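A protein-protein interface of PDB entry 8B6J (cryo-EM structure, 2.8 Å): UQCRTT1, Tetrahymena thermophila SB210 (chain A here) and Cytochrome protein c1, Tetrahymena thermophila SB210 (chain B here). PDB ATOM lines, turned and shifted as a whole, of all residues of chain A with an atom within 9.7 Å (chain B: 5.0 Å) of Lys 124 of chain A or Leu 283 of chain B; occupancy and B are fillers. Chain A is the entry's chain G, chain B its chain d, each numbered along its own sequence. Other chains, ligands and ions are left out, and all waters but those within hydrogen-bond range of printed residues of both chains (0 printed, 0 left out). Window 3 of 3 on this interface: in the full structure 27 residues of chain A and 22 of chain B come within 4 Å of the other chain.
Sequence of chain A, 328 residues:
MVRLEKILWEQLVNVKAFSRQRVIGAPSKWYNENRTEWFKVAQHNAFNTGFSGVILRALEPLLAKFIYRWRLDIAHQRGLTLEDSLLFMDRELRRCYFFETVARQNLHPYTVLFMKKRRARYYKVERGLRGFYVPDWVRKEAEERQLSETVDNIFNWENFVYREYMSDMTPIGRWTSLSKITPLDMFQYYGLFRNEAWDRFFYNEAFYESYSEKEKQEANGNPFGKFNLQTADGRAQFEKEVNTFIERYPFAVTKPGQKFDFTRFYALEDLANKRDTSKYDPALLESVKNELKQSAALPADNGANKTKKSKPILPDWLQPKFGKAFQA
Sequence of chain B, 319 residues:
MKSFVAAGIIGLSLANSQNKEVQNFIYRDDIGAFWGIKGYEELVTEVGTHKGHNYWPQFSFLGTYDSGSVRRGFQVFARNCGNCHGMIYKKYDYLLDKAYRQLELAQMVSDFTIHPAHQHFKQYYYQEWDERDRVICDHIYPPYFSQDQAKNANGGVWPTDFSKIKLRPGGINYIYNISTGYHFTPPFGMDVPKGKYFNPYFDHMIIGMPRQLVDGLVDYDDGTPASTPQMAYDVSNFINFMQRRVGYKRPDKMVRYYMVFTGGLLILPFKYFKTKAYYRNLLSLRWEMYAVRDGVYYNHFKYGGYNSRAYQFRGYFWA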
ATOM      1  N   ARG A  78     -19.944  34.213 -21.163  1.00  0.00           N
ATOM      2  CA  ARG A  78     -20.492  33.482 -22.296  1.00  0.00           C
ATOM      3  C   ARG A  78     -21.146  34.393 -23.325  1.00  0.00           C
ATOM      4  O   ARG A  78     -21.824  33.900 -24.230  1.00  0.00           O
ATOM      5  CB  ARG A  78     -21.502  32.446 -21.804  1.00  0.00           C
ATOM      6  CG  ARG A  78     -20.982  31.576 -20.675  1.00  0.00           C
ATOM      7  CD  ARG A  78     -21.973  30.494 -20.303  1.00  0.00           C
ATOM      8  NE  ARG A  78     -21.525  29.723 -19.149  1.00  0.00           N
ATOM      9  CZ  ARG A  78     -22.147  28.653 -18.676  1.00  0.00           C
ATOM     10  NH1 ARG A  78     -23.246  28.184 -19.242  1.00  0.00           N
ATOM     11  NH2 ARG A  78     -21.652  28.036 -17.607  1.00  0.00           N
ATOM     12  N   LYS A 116     -31.864  31.048 -28.423  1.00  0.00           N
ATOM     13  CA  LYS A 116     -31.147  29.791 -28.609  1.00  0.00           C
ATOM     14  C   LYS A 116     -29.821  30.002 -29.333  1.00  0.00           C
ATOM     15  O   LYS A 116     -28.813  29.373 -28.990  1.00  0.00           O
ATOM     16  CB  LYS A 116     -32.026  28.800 -29.370  1.00  0.00           C
ATOM     17  CG  LYS A 116     -33.257  28.357 -28.597  1.00  0.00           C
ATOM     18  CD  LYS A 116     -34.043  27.304 -29.355  1.00  0.00           C
ATOM     19  CE  LYS A 116     -35.177  26.749 -28.514  1.00  0.00           C
ATOM     20  NZ  LYS A 116     -35.921  25.671 -29.219  1.00  0.00           N
ATOM     21  N   LYS A 117     -29.796  30.887 -30.331  1.00  0.00           N
ATOM     22  CA  LYS A 117     -28.571  31.099 -31.095  1.00  0.00           C
ATOM     23  C   LYS A 117     -27.493  31.780 -30.264  1.00  0.00           C
ATOM     24  O   LYS A 117     -26.301  31.531 -30.476  1.00  0.00           O
ATOM     25  CB  LYS A 117     -28.869  31.921 -32.349  1.00  0.00           C
ATOM     26  CG  LYS A 117     -29.675  31.180 -33.403  1.00  0.00           C
ATOM     27  CD  LYS A 117     -28.896  30.010 -33.985  1.00  0.00           C
ATOM     28  CE  LYS A 117     -29.666  29.326 -35.099  1.00  0.00           C
ATOM     29  NZ  LYS A 117     -28.911  28.178 -35.670  1.00  0.00           N
ATOM     30  N   ARG A 118     -27.882  32.642 -29.323  1.00  0.00           N
ATOM     31  CA  ARG A 118     -26.887  33.282 -28.469  1.00  0.00           C
ATOM     32  C   ARG A 118     -26.108  32.245 -27.670  1.00  0.00           C
ATOM     33  O   ARG A 118     -24.888  32.362 -27.511  1.00  0.00           O
ATOM     34  CB  ARG A 118     -27.563  34.285 -27.538  1.00  0.00           C
ATOM     35  CG  ARG A 118     -27.781  35.655 -28.155  1.00  0.00           C
ATOM     36  CD  ARG A 118     -28.571  36.550 -27.224  1.00  0.00           C
ATOM     37  NE  ARG A 118     -30.008  36.390 -27.400  1.00  0.00           N
ATOM     38  CZ  ARG A 118     -30.919  36.718 -26.495  1.00  0.00           C
ATOM     39  NH1 ARG A 118     -30.575  37.189 -25.307  1.00  0.00           N
ATOM     40  NH2 ARG A 118     -32.208  36.562 -26.783  1.00  0.00           N
ATOM     41  N   ARG A 119     -26.797  31.226 -27.155  1.00  0.00           N
ATOM     42  CA  ARG A 119     -26.100  30.149 -26.461  1.00  0.00           C
ATOM     43  C   ARG A 119     -25.377  29.229 -27.436  1.00  0.00           C
ATOM     44  O   ARG A 119     -24.319  28.683 -27.099  1.00  0.00           O
ATOM     45  CB  ARG A 119     -27.083  29.345 -25.612  1.00  0.00           C
ATOM     46  CG  ARG A 119     -27.531  30.056 -24.349  1.00  0.00           C
ATOM     47  CD  ARG A 119     -28.177  29.091 -23.375  1.00  0.00           C
ATOM     48  NE  ARG A 119     -28.356  29.677 -22.054  1.00  0.00           N
ATOM     49  CZ  ARG A 119     -29.403  30.402 -21.687  1.00  0.00           C
ATOM     50  NH1 ARG A 119     -30.391  30.668 -22.526  1.00  0.00           N
ATOM     51  NH2 ARG A 119     -29.460  30.876 -20.445  1.00  0.00           N
ATOM     52  N   ALA A 120     -25.936  29.035 -28.634  1.00  0.00           N
ATOM     53  CA  ALA A 120     -25.283  28.181 -29.621  1.00  0.00           C
ATOM     54  C   ALA A 120     -23.913  28.725 -29.994  1.00  0.00           C
ATOM     55  O   ALA A 120     -22.945  27.963 -30.115  1.00  0.00           O
ATOM     56  CB  ALA A 120     -26.164  28.046 -30.861  1.00  0.00           C
ATOM     57  N   ARG A 121     -23.813  30.045 -30.183  1.00  0.00           N
ATOM     58  CA  ARG A 121     -22.525  30.684 -30.429  1.00  0.00           C
ATOM     59  C   ARG A 121     -21.457  30.122 -29.505  1.00  0.00           C
ATOM     60  O   ARG A 121     -20.463  29.534 -29.945  1.00  0.00           O
ATOM     61  CB  ARG A 121     -22.615  32.193 -30.190  1.00  0.00           C
ATOM     62  CG  ARG A 121     -23.431  33.021 -31.145  1.00  0.00           C
ATOM     63  CD  ARG A 121     -23.403  34.455 -30.635  1.00  0.00           C
ATOM     64  NE  ARG A 121     -24.092  35.410 -31.489  1.00  0.00           N
ATOM     65  CZ  ARG A 121     -24.204  36.703 -31.214  1.00  0.00           C
ATOM     66  NH1 ARG A 121     -23.684  37.223 -30.114  1.00  0.00           N
ATOM     67  NH2 ARG A 121     -24.852  37.494 -32.063  1.00  0.00           N
ATOM     68  N   TYR A 122     -21.669  30.308 -28.203  1.00  0.00           N
ATOM     69  CA  TYR A 122     -20.666  29.939 -27.215  1.00  0.00           C
ATOM     70  C   TYR A 122     -20.479  28.430 -27.147  1.00  0.00           C
ATOM     71  O   TYR A 122     -19.345  27.945 -27.070  1.00  0.00           O
ATOM     72  CB  TYR A 122     -21.066  30.493 -25.848  1.00  0.00           C
ATOM     73  CG  TYR A 122     -20.148  30.095 -24.720  1.00  0.00           C
ATOM     74  CD1 TYR A 122     -18.969  30.784 -24.484  1.00  0.00           C
ATOM     75  CD2 TYR A 122     -20.465  29.036 -23.883  1.00  0.00           C
ATOM     76  CE1 TYR A 122     -18.129  30.426 -23.451  1.00  0.00           C
ATOM     77  CE2 TYR A 122     -19.632  28.671 -22.849  1.00  0.00           C
ATOM     78  CZ  TYR A 122     -18.465  29.370 -22.636  1.00  0.00           C
ATOM     79  OH  TYR A 122     -17.631  29.008 -21.605  1.00  0.00           O
ATOM     80  N   TYR A 123     -21.572  27.666 -27.176  1.00  0.00           N
ATOM     81  CA  TYR A 123     -21.454  26.244 -26.888  1.00  0.00           C
ATOM     82  C   TYR A 123     -20.852  25.458 -28.044  1.00  0.00           C
ATOM     83  O   TYR A 123     -20.205  24.432 -27.807  1.00  0.00           O
ATOM     84  CB  TYR A 123     -22.813  25.675 -26.489  1.00  0.00           C
ATOM     85  CG  TYR A 123     -23.119  25.920 -25.031  1.00  0.00           C
ATOM     86  CD1 TYR A 123     -22.493  25.177 -24.040  1.00  0.00           C
ATOM     87  CD2 TYR A 123     -24.013  26.905 -24.643  1.00  0.00           C
ATOM     88  CE1 TYR A 123     -22.757  25.401 -22.708  1.00  0.00           C
ATOM     89  CE2 TYR A 123     -24.285  27.135 -23.310  1.00  0.00           C
ATOM     90  CZ  TYR A 123     -23.654  26.381 -22.348  1.00  0.00           C
ATOM     91  OH  TYR A 123     -23.922  26.607 -21.019  1.00  0.00           O
ATOM     92  N   LYS A 124     -21.015  25.922 -29.286  1.00  0.00           N
ATOM     93  CA  LYS A 124     -20.330  25.268 -30.396  1.00  0.00           C
ATOM     94  C   LYS A 124     -18.830  25.199 -30.139  1.00  0.00           C
ATOM     95  O   LYS A 124     -18.180  24.198 -30.459  1.00  0.00           O
ATOM     96  CB  LYS A 124     -20.612  26.009 -31.703  1.00  0.00           C
ATOM     97  CG  LYS A 124     -19.935  25.390 -32.918  1.00  0.00           C
ATOM     98  CD  LYS A 124     -20.269  26.136 -34.197  1.00  0.00           C
ATOM     99  CE  LYS A 124     -19.620  27.507 -34.233  1.00  0.00           C
ATOM    100  NZ  LYS A 124     -19.849  28.191 -35.533  1.00  0.00           N
ATOM    101  N   VAL A 125     -18.267  26.258 -29.558  1.00  0.00           N
ATOM    102  CA  VAL A 125     -16.843  26.277 -29.244  1.00  0.00           C
ATOM    103  C   VAL A 125     -16.573  25.576 -27.920  1.00  0.00           C
ATOM    104  O   VAL A 125     -15.570  24.870 -27.772  1.00  0.00           O
ATOM    105  CB  VAL A 125     -16.331  27.727 -29.229  1.00  0.00           C
ATOM    106  CG1 VAL A 125     -14.866  27.769 -28.833  1.00  0.00           C
ATOM    107  CG2 VAL A 125     -16.543  28.382 -30.584  1.00  0.00           C
ATOM    108  N   GLU A 126     -17.458  25.758 -26.937  1.00  0.00           N
ATOM    109  CA  GLU A 126     -17.229  25.179 -25.618  1.00  0.00           C
ATOM    110  C   GLU A 126     -17.143  23.660 -25.687  1.00  0.00           C
ATOM    111  O   GLU A 126     -16.272  23.052 -25.055  1.00  0.00           O
ATOM    112  CB  GLU A 126     -18.340  25.606 -24.660  1.00  0.00           C
ATOM    113  CG  GLU A 126     -18.190  25.074 -23.240  1.00  0.00           C
ATOM    114  CD  GLU A 126     -16.964  25.615 -22.537  1.00  0.00           C
ATOM    115  OE1 GLU A 126     -16.322  26.535 -23.084  1.00  0.00           O
ATOM    116  OE2 GLU A 126     -16.642  25.123 -21.435  1.00  0.00           O
ATOM    117  N   ARG A 127     -18.040  23.026 -26.445  1.00  0.00           N
ATOM    118  CA  ARG A 127     -17.984  21.574 -26.575  1.00  0.00           C
ATOM    119  C   ARG A 127     -16.693  21.137 -27.254  1.00  0.00           C
ATOM    120  O   ARG A 127     -16.075  20.146 -26.849  1.00  0.00           O
ATOM    121  CB  ARG A 127     -19.201  21.064 -27.346  1.00  0.00           C
ATOM    122  CG  ARG A 127     -20.382  20.690 -26.458  1.00  0.00           C
ATOM    123  CD  ARG A 127     -21.014  21.904 -25.802  1.00  0.00           C
ATOM    124  NE  ARG A 127     -21.342  21.662 -24.402  1.00  0.00           N
ATOM    125  CZ  ARG A 127     -22.487  21.149 -23.972  1.00  0.00           C
ATOM    126  NH1 ARG A 127     -23.447  20.794 -24.810  1.00  0.00           N
ATOM    127  NH2 ARG A 127     -22.673  20.986 -22.665  1.00  0.00           N
ATOM    128  N   GLY A 128     -16.271  21.861 -28.293  1.00  0.00           N
ATOM    129  CA  GLY A 128     -15.009  21.538 -28.938  1.00  0.00           C
ATOM    130  C   GLY A 128     -13.821  21.743 -28.019  1.00  0.00           C
ATOM    131  O   GLY A 128     -12.937  20.888 -27.923  1.00  0.00           O
ATOM    132  N   LEU A 129     -13.786  22.881 -27.327  1.00  0.00           N
ATOM    133  CA  LEU A 129     -12.727  23.189 -26.373  1.00  0.00           C
ATOM    134  C   LEU A 129     -13.351  23.836 -25.149  1.00  0.00           C
ATOM    135  O   LEU A 129     -14.001  24.878 -25.263  1.00  0.00           O
ATOM    136  CB  LEU A 129     -11.674  24.119 -26.982  1.00  0.00           C
ATOM    137  CG  LEU A 129     -10.415  23.471 -27.560  1.00  0.00           C
ATOM    138  CD1 LEU A 129      -9.515  24.534 -28.156  1.00  0.00           C
ATOM    139  CD2 LEU A 129      -9.668  22.676 -26.500  1.00  0.00           C
ATOM    140  N   ARG A 130     -13.147  23.227 -23.986  1.00  0.00           N
ATOM    141  CA  ARG A 130     -13.694  23.765 -22.753  1.00  0.00           C
ATOM    142  C   ARG A 130     -12.863  24.949 -22.269  1.00  0.00           C
ATOM    143  O   ARG A 130     -11.697  25.117 -22.633  1.00  0.00           O
ATOM    144  CB  ARG A 130     -13.749  22.685 -21.676  1.00  0.00           C
ATOM    145  CG  ARG A 130     -14.575  21.472 -22.063  1.00  0.00           C
ATOM    146  CD  ARG A 130     -15.132  20.779 -20.836  1.00  0.00           C
ATOM    147  NE  ARG A 130     -16.086  21.629 -20.134  1.00  0.00           N
ATOM    148  CZ  ARG A 130     -16.539  21.397 -18.910  1.00  0.00           C
ATOM    149  NH1 ARG A 130     -16.137  20.350 -18.211  1.00  0.00           N
ATOM    150  NH2 ARG A 130     -17.414  22.242 -18.372  1.00  0.00           N
ATOM    151  N   PHE A 132     -13.833  28.153 -22.800  1.00  0.00           N
ATOM    152  CA  PHE A 132     -13.931  29.243 -23.758  1.00  0.00           C
ATOM    153  C   PHE A 132     -14.309  30.540 -23.055  1.00  0.00           C
ATOM    154  O   PHE A 132     -15.246  30.574 -22.251  1.00  0.00           O
ATOM    155  CB  PHE A 132     -14.962  28.904 -24.834  1.00  0.00           C
ATOM    156  CG  PHE A 132     -15.101  29.953 -25.903  1.00  0.00           C
ATOM    157  CD1 PHE A 132     -14.024  30.741 -26.273  1.00  0.00           C
ATOM    158  CD2 PHE A 132     -16.315  30.152 -26.536  1.00  0.00           C
ATOM    159  CE1 PHE A 132     -14.157  31.702 -27.253  1.00  0.00           C
ATOM    160  CE2 PHE A 132     -16.451  31.113 -27.517  1.00  0.00           C
ATOM    161  CZ  PHE A 132     -15.371  31.888 -27.875  1.00  0.00           C
ATOM    162  N   TYR B 279     -14.953  15.027 -32.092  1.00  0.00           N
ATOM    163  CA  TYR B 279     -16.047  15.949 -31.802  1.00  0.00           C
ATOM    164  C   TYR B 279     -15.668  17.373 -32.180  1.00  0.00           C
ATOM    165  O   TYR B 279     -16.479  18.110 -32.752  1.00  0.00           O
ATOM    166  CB  TYR B 279     -16.427  15.880 -30.324  1.00  0.00           C
ATOM    167  CG  TYR B 279     -16.862  14.514 -29.848  1.00  0.00           C
ATOM    168  CD1 TYR B 279     -17.332  13.560 -30.738  1.00  0.00           C
ATOM    169  CD2 TYR B 279     -16.796  14.178 -28.503  1.00  0.00           C
ATOM    170  CE1 TYR B 279     -17.725  12.311 -30.302  1.00  0.00           C
ATOM    171  CE2 TYR B 279     -17.186  12.933 -28.058  1.00  0.00           C
ATOM    172  CZ  TYR B 279     -17.650  12.003 -28.960  1.00  0.00           C
ATOM    173  OH  TYR B 279     -18.040  10.761 -28.520  1.00  0.00           O
ATOM    174  N   ARG B 280     -14.437  17.781 -31.866  1.00  0.00           N
ATOM    175  CA  ARG B 280     -13.995  19.120 -32.238  1.00  0.00           C
ATOM    176  C   ARG B 280     -14.018  19.300 -33.751  1.00  0.00           C
ATOM    177  O   ARG B 280     -14.351  20.379 -34.253  1.00  0.00           O
ATOM    178  CB  ARG B 280     -12.597  19.386 -31.677  1.00  0.00           C
ATOM    179  CG  ARG B 280     -12.028  20.741 -32.052  1.00  0.00           C
ATOM    180  CD  ARG B 280     -11.023  21.247 -31.023  1.00  0.00           C
ATOM    181  NE  ARG B 280      -9.967  20.281 -30.737  1.00  0.00           N
ATOM    182  CZ  ARG B 280      -9.924  19.492 -29.671  1.00  0.00           C
ATOM    183  NH1 ARG B 280     -10.876  19.514 -28.752  1.00  0.00           N
ATOM    184  NH2 ARG B 280      -8.898  18.661 -29.520  1.00  0.00           N
ATOM    185  N   ASN B 281     -13.664  18.251 -34.497  1.00  0.00           N
ATOM    186  CA  ASN B 281     -13.754  18.312 -35.952  1.00  0.00           C
ATOM    187  C   ASN B 281     -15.200  18.461 -36.410  1.00  0.00           C
ATOM    188  O   ASN B 281     -15.490  19.234 -37.329  1.00  0.00           O
ATOM    189  CB  ASN B 281     -13.132  17.061 -36.573  1.00  0.00           C
ATOM    190  CG  ASN B 281     -11.620  17.074 -36.522  1.00  0.00           C
ATOM    191  OD1 ASN B 281     -10.999  18.134 -36.468  1.00  0.00           O
ATOM    192  ND2 ASN B 281     -11.019  15.892 -36.546  1.00  0.00           N
ATOM    193  N   LEU B 282     -16.120  17.721 -35.786  1.00  0.00           N
ATOM    194  CA  LEU B 282     -17.518  17.785 -36.202  1.00  0.00           C
ATOM    195  C   LEU B 282     -18.146  19.134 -35.881  1.00  0.00           C
ATOM    196  O   LEU B 282     -19.095  19.548 -36.555  1.00  0.00           O
ATOM    197  CB  LEU B 282     -18.321  16.668 -35.535  1.00  0.00           C
ATOM    198  CG  LEU B 282     -18.095  15.243 -36.045  1.00  0.00           C
ATOM    199  CD1 LEU B 282     -18.980  14.276 -35.281  1.00  0.00           C
ATOM    200  CD2 LEU B 282     -18.358  15.141 -37.539  1.00  0.00           C
ATOM    201  N   LEU B 283     -17.640  19.828 -34.866  1.00  0.00           N
ATOM    202  CA  LEU B 283     -18.201  21.107 -34.450  1.00  0.00           C
ATOM    203  C   LEU B 283     -17.718  22.274 -35.300  1.00  0.00           C
ATOM    204  O   LEU B 283     -18.188  23.398 -35.096  1.00  0.00           O
ATOM    205  CB  LEU B 283     -17.863  21.366 -32.981  1.00  0.00           C
ATOM    206  CG  LEU B 283     -18.521  20.406 -31.990  1.00  0.00           C
ATOM    207  CD1 LEU B 283     -17.844  20.489 -30.637  1.00  0.00           C
ATOM    208  CD2 LEU B 283     -20.004  20.709 -31.863  1.00  0.00           C
ATOM    209  N   SER B 284     -16.801  22.042 -36.238  1.00  0.00           N
ATOM    210  CA  SER B 284     -16.293  23.099 -37.112  1.00  0.00           C
ATOM    211  C   SER B 284     -17.351  23.394 -38.170  1.00  0.00           C
ATOM    212  O   SER B 284     -17.281  22.950 -39.319  1.00  0.00           O
ATOM    213  CB  SER B 284     -14.970  22.685 -37.738  1.00  0.00           C
ATOM    214  OG  SER B 284     -14.042  22.284 -36.745  1.00  0.00           O
ATOM    215  N   LEU B 285     -18.354  24.167 -37.765  1.00  0.00           N
ATOM    216  CA  LEU B 285     -19.494  24.498 -38.606  1.00  0.00           C
ATOM    217  C   LEU B 285     -19.506  25.988 -38.917  1.00  0.00           C
ATOM    218  O   LEU B 285     -18.990  26.805 -38.150  1.00  0.00           O
ATOM    219  CB  LEU B 285     -20.812  24.121 -37.923  1.00  0.00           C
ATOM    220  CG  LEU B 285     -20.994  22.663 -37.503  1.00  0.00           C
ATOM    221  CD1 LEU B 285     -22.287  22.504 -36.724  1.00  0.00           C
ATOM    222  CD2 LEU B 285     -20.982  21.746 -38.710  1.00  0.00           C
ATOM    223  N   ARG B 286     -20.100  26.330 -40.054  1.00  0.00           N
ATOM    224  CA  ARG B 286     -20.385  27.710 -40.410  1.00  0.00           C
ATOM    225  C   ARG B 286     -21.893  27.911 -40.438  1.00  0.00           C
ATOM    226  O   ARG B 286     -22.629  27.071 -40.962  1.00  0.00           O
ATOM    227  CB  ARG B 286     -19.786  28.076 -41.770  1.00  0.00           C
ATOM    228  CG  ARG B 286     -19.805  29.566 -42.053  1.00  0.00           C
ATOM    229  CD  ARG B 286     -19.502  29.880 -43.504  1.00  0.00           C
ATOM    230  NE  ARG B 286     -18.184  29.417 -43.922  1.00  0.00           N
ATOM    231  CZ  ARG B 286     -17.041  29.978 -43.557  1.00  0.00           C
ATOM    232  NH1 ARG B 286     -17.006  30.991 -42.708  1.00  0.00           N
ATOM    233  NH2 ARG B 286     -15.900  29.510 -44.055  1.00  0.00           N
ATOM    234  N   TRP B 287     -22.347  29.022 -39.870  1.00  0.00           N
ATOM    235  CA  TRP B 287     -23.761  29.349 -39.801  1.00  0.00           C
ATOM    236  C   TRP B 287     -24.009  30.694 -40.465  1.00  0.00           C
ATOM    237  O   TRP B 287     -23.156  31.584 -40.439  1.00  0.00           O
ATOM    238  CB  TRP B 287     -24.250  29.383 -38.351  1.00  0.00           C
ATOM    239  CG  TRP B 287     -24.211  28.050 -37.675  1.00  0.00           C
ATOM    240  CD1 TRP B 287     -24.218  26.826 -38.274  1.00  0.00           C
ATOM    241  CD2 TRP B 287     -24.150  27.807 -36.266  1.00  0.00           C
ATOM    242  NE1 TRP B 287     -24.172  25.835 -37.326  1.00  0.00           N
ATOM    243  CE2 TRP B 287     -24.129  26.412 -36.085  1.00  0.00           C
ATOM    244  CE3 TRP B 287     -24.115  28.633 -35.140  1.00  0.00           C
ATOM    245  CZ2 TRP B 287     -24.073  25.825 -34.825  1.00  0.00           C
ATOM    246  CZ3 TRP B 287     -24.060  28.049 -33.891  1.00  0.00           C
ATOM    247  CH2 TRP B 287     -24.039  26.659 -33.743  1.00  0.00           C
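The guanidinium group (NH1) of Arg 280 of chain B lies within hydrogen-bond range of the backbone carbonyl oxygen (O) of Gly 128 of chain A, at 2.6 Å. The backbone carbonyl oxygen (O) of Leu 285 of chain B is in hydrogen-bond range of the side-chain amino group (NZ) of Lys 124 of chain A (3.1 Å).
The side-chain hydroxyl (OG) of Ser 284 of chain B is in hydrogen-bond range of the backbone carbonyl oxygen (O) of Arg 280 of chain B, at 3.2 Å.
Among the printed residues, merely in contact across the chains: Gly 128 of chain A with Leu 283 of chain B (3.1 Å), Lys 124 of chain A with Leu 283 of chain B (3.4 Å), Arg 127 of chain A with Leu 283 of chain B (3.6 Å), Ala 120 of chain A with Trp 287 of chain B (3.7 Å) and Lys 124 of chain A with Trp 287 of chain B (3.8 Å).
Of the printed residues of chain B, Ala 120 of chain A touches Trp 287 (3.7 Å). Tyr 123 of chain A touches none of the printed residues of chain B. Lys 124 of chain A touches just these residues of chain B: Leu 283 (3.4 Å), Leu 285 (3.1 Å) and Trp 287 (3.8 Å). Of the printed residues of chain B, Arg 127 of chain A touches Leu 283 (3.6 Å). Of the printed residues of chain B, Gly 128 of chain A touches Arg 280 (2.6 Å) and Leu 283 (3.1 Å). Phe 132 of chain A touches none of the printed residues of chain B. Leu 283 of chain B touches just these residues of chain A: Lys 124, Arg 127 and Gly 128. Leu 285 of chain B touches just one residue of chain A: Lys 124 (3.1 Å). Of the printed residues of chain A, Trp 287 of chain B touches Ala 120 and Lys 124. The nearest residue of chain B that does not touch Lys 124 of chain A is Arg 286 of chain B (4.9 Å). The nearest residue of chain A that does not touch Leu 283 of chain B is Tyr 123 of chain A (5.4 Å). The nearest printed residue of chain B that does not touch Arg 127 of chain A is Tyr 279 of chain B (5.5 Å).
Printed residues of chain A that touch a printed residue of chain B: Ala 120, Lys 124, Arg 127 and Gly 128. Printed residues of chain B that touch a printed residue of chain A: Arg 280, Leu 283, Leu 285 and Trp 287. Hydrophobic or aromatic side chains of chain B that line the printed part of chain A: Leu 283 and Trp 287. Along chain B the printed residues that touch a printed residue of chain A span positions 280 to 287. Among the printed residues, 7 pairs touch across the chains.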
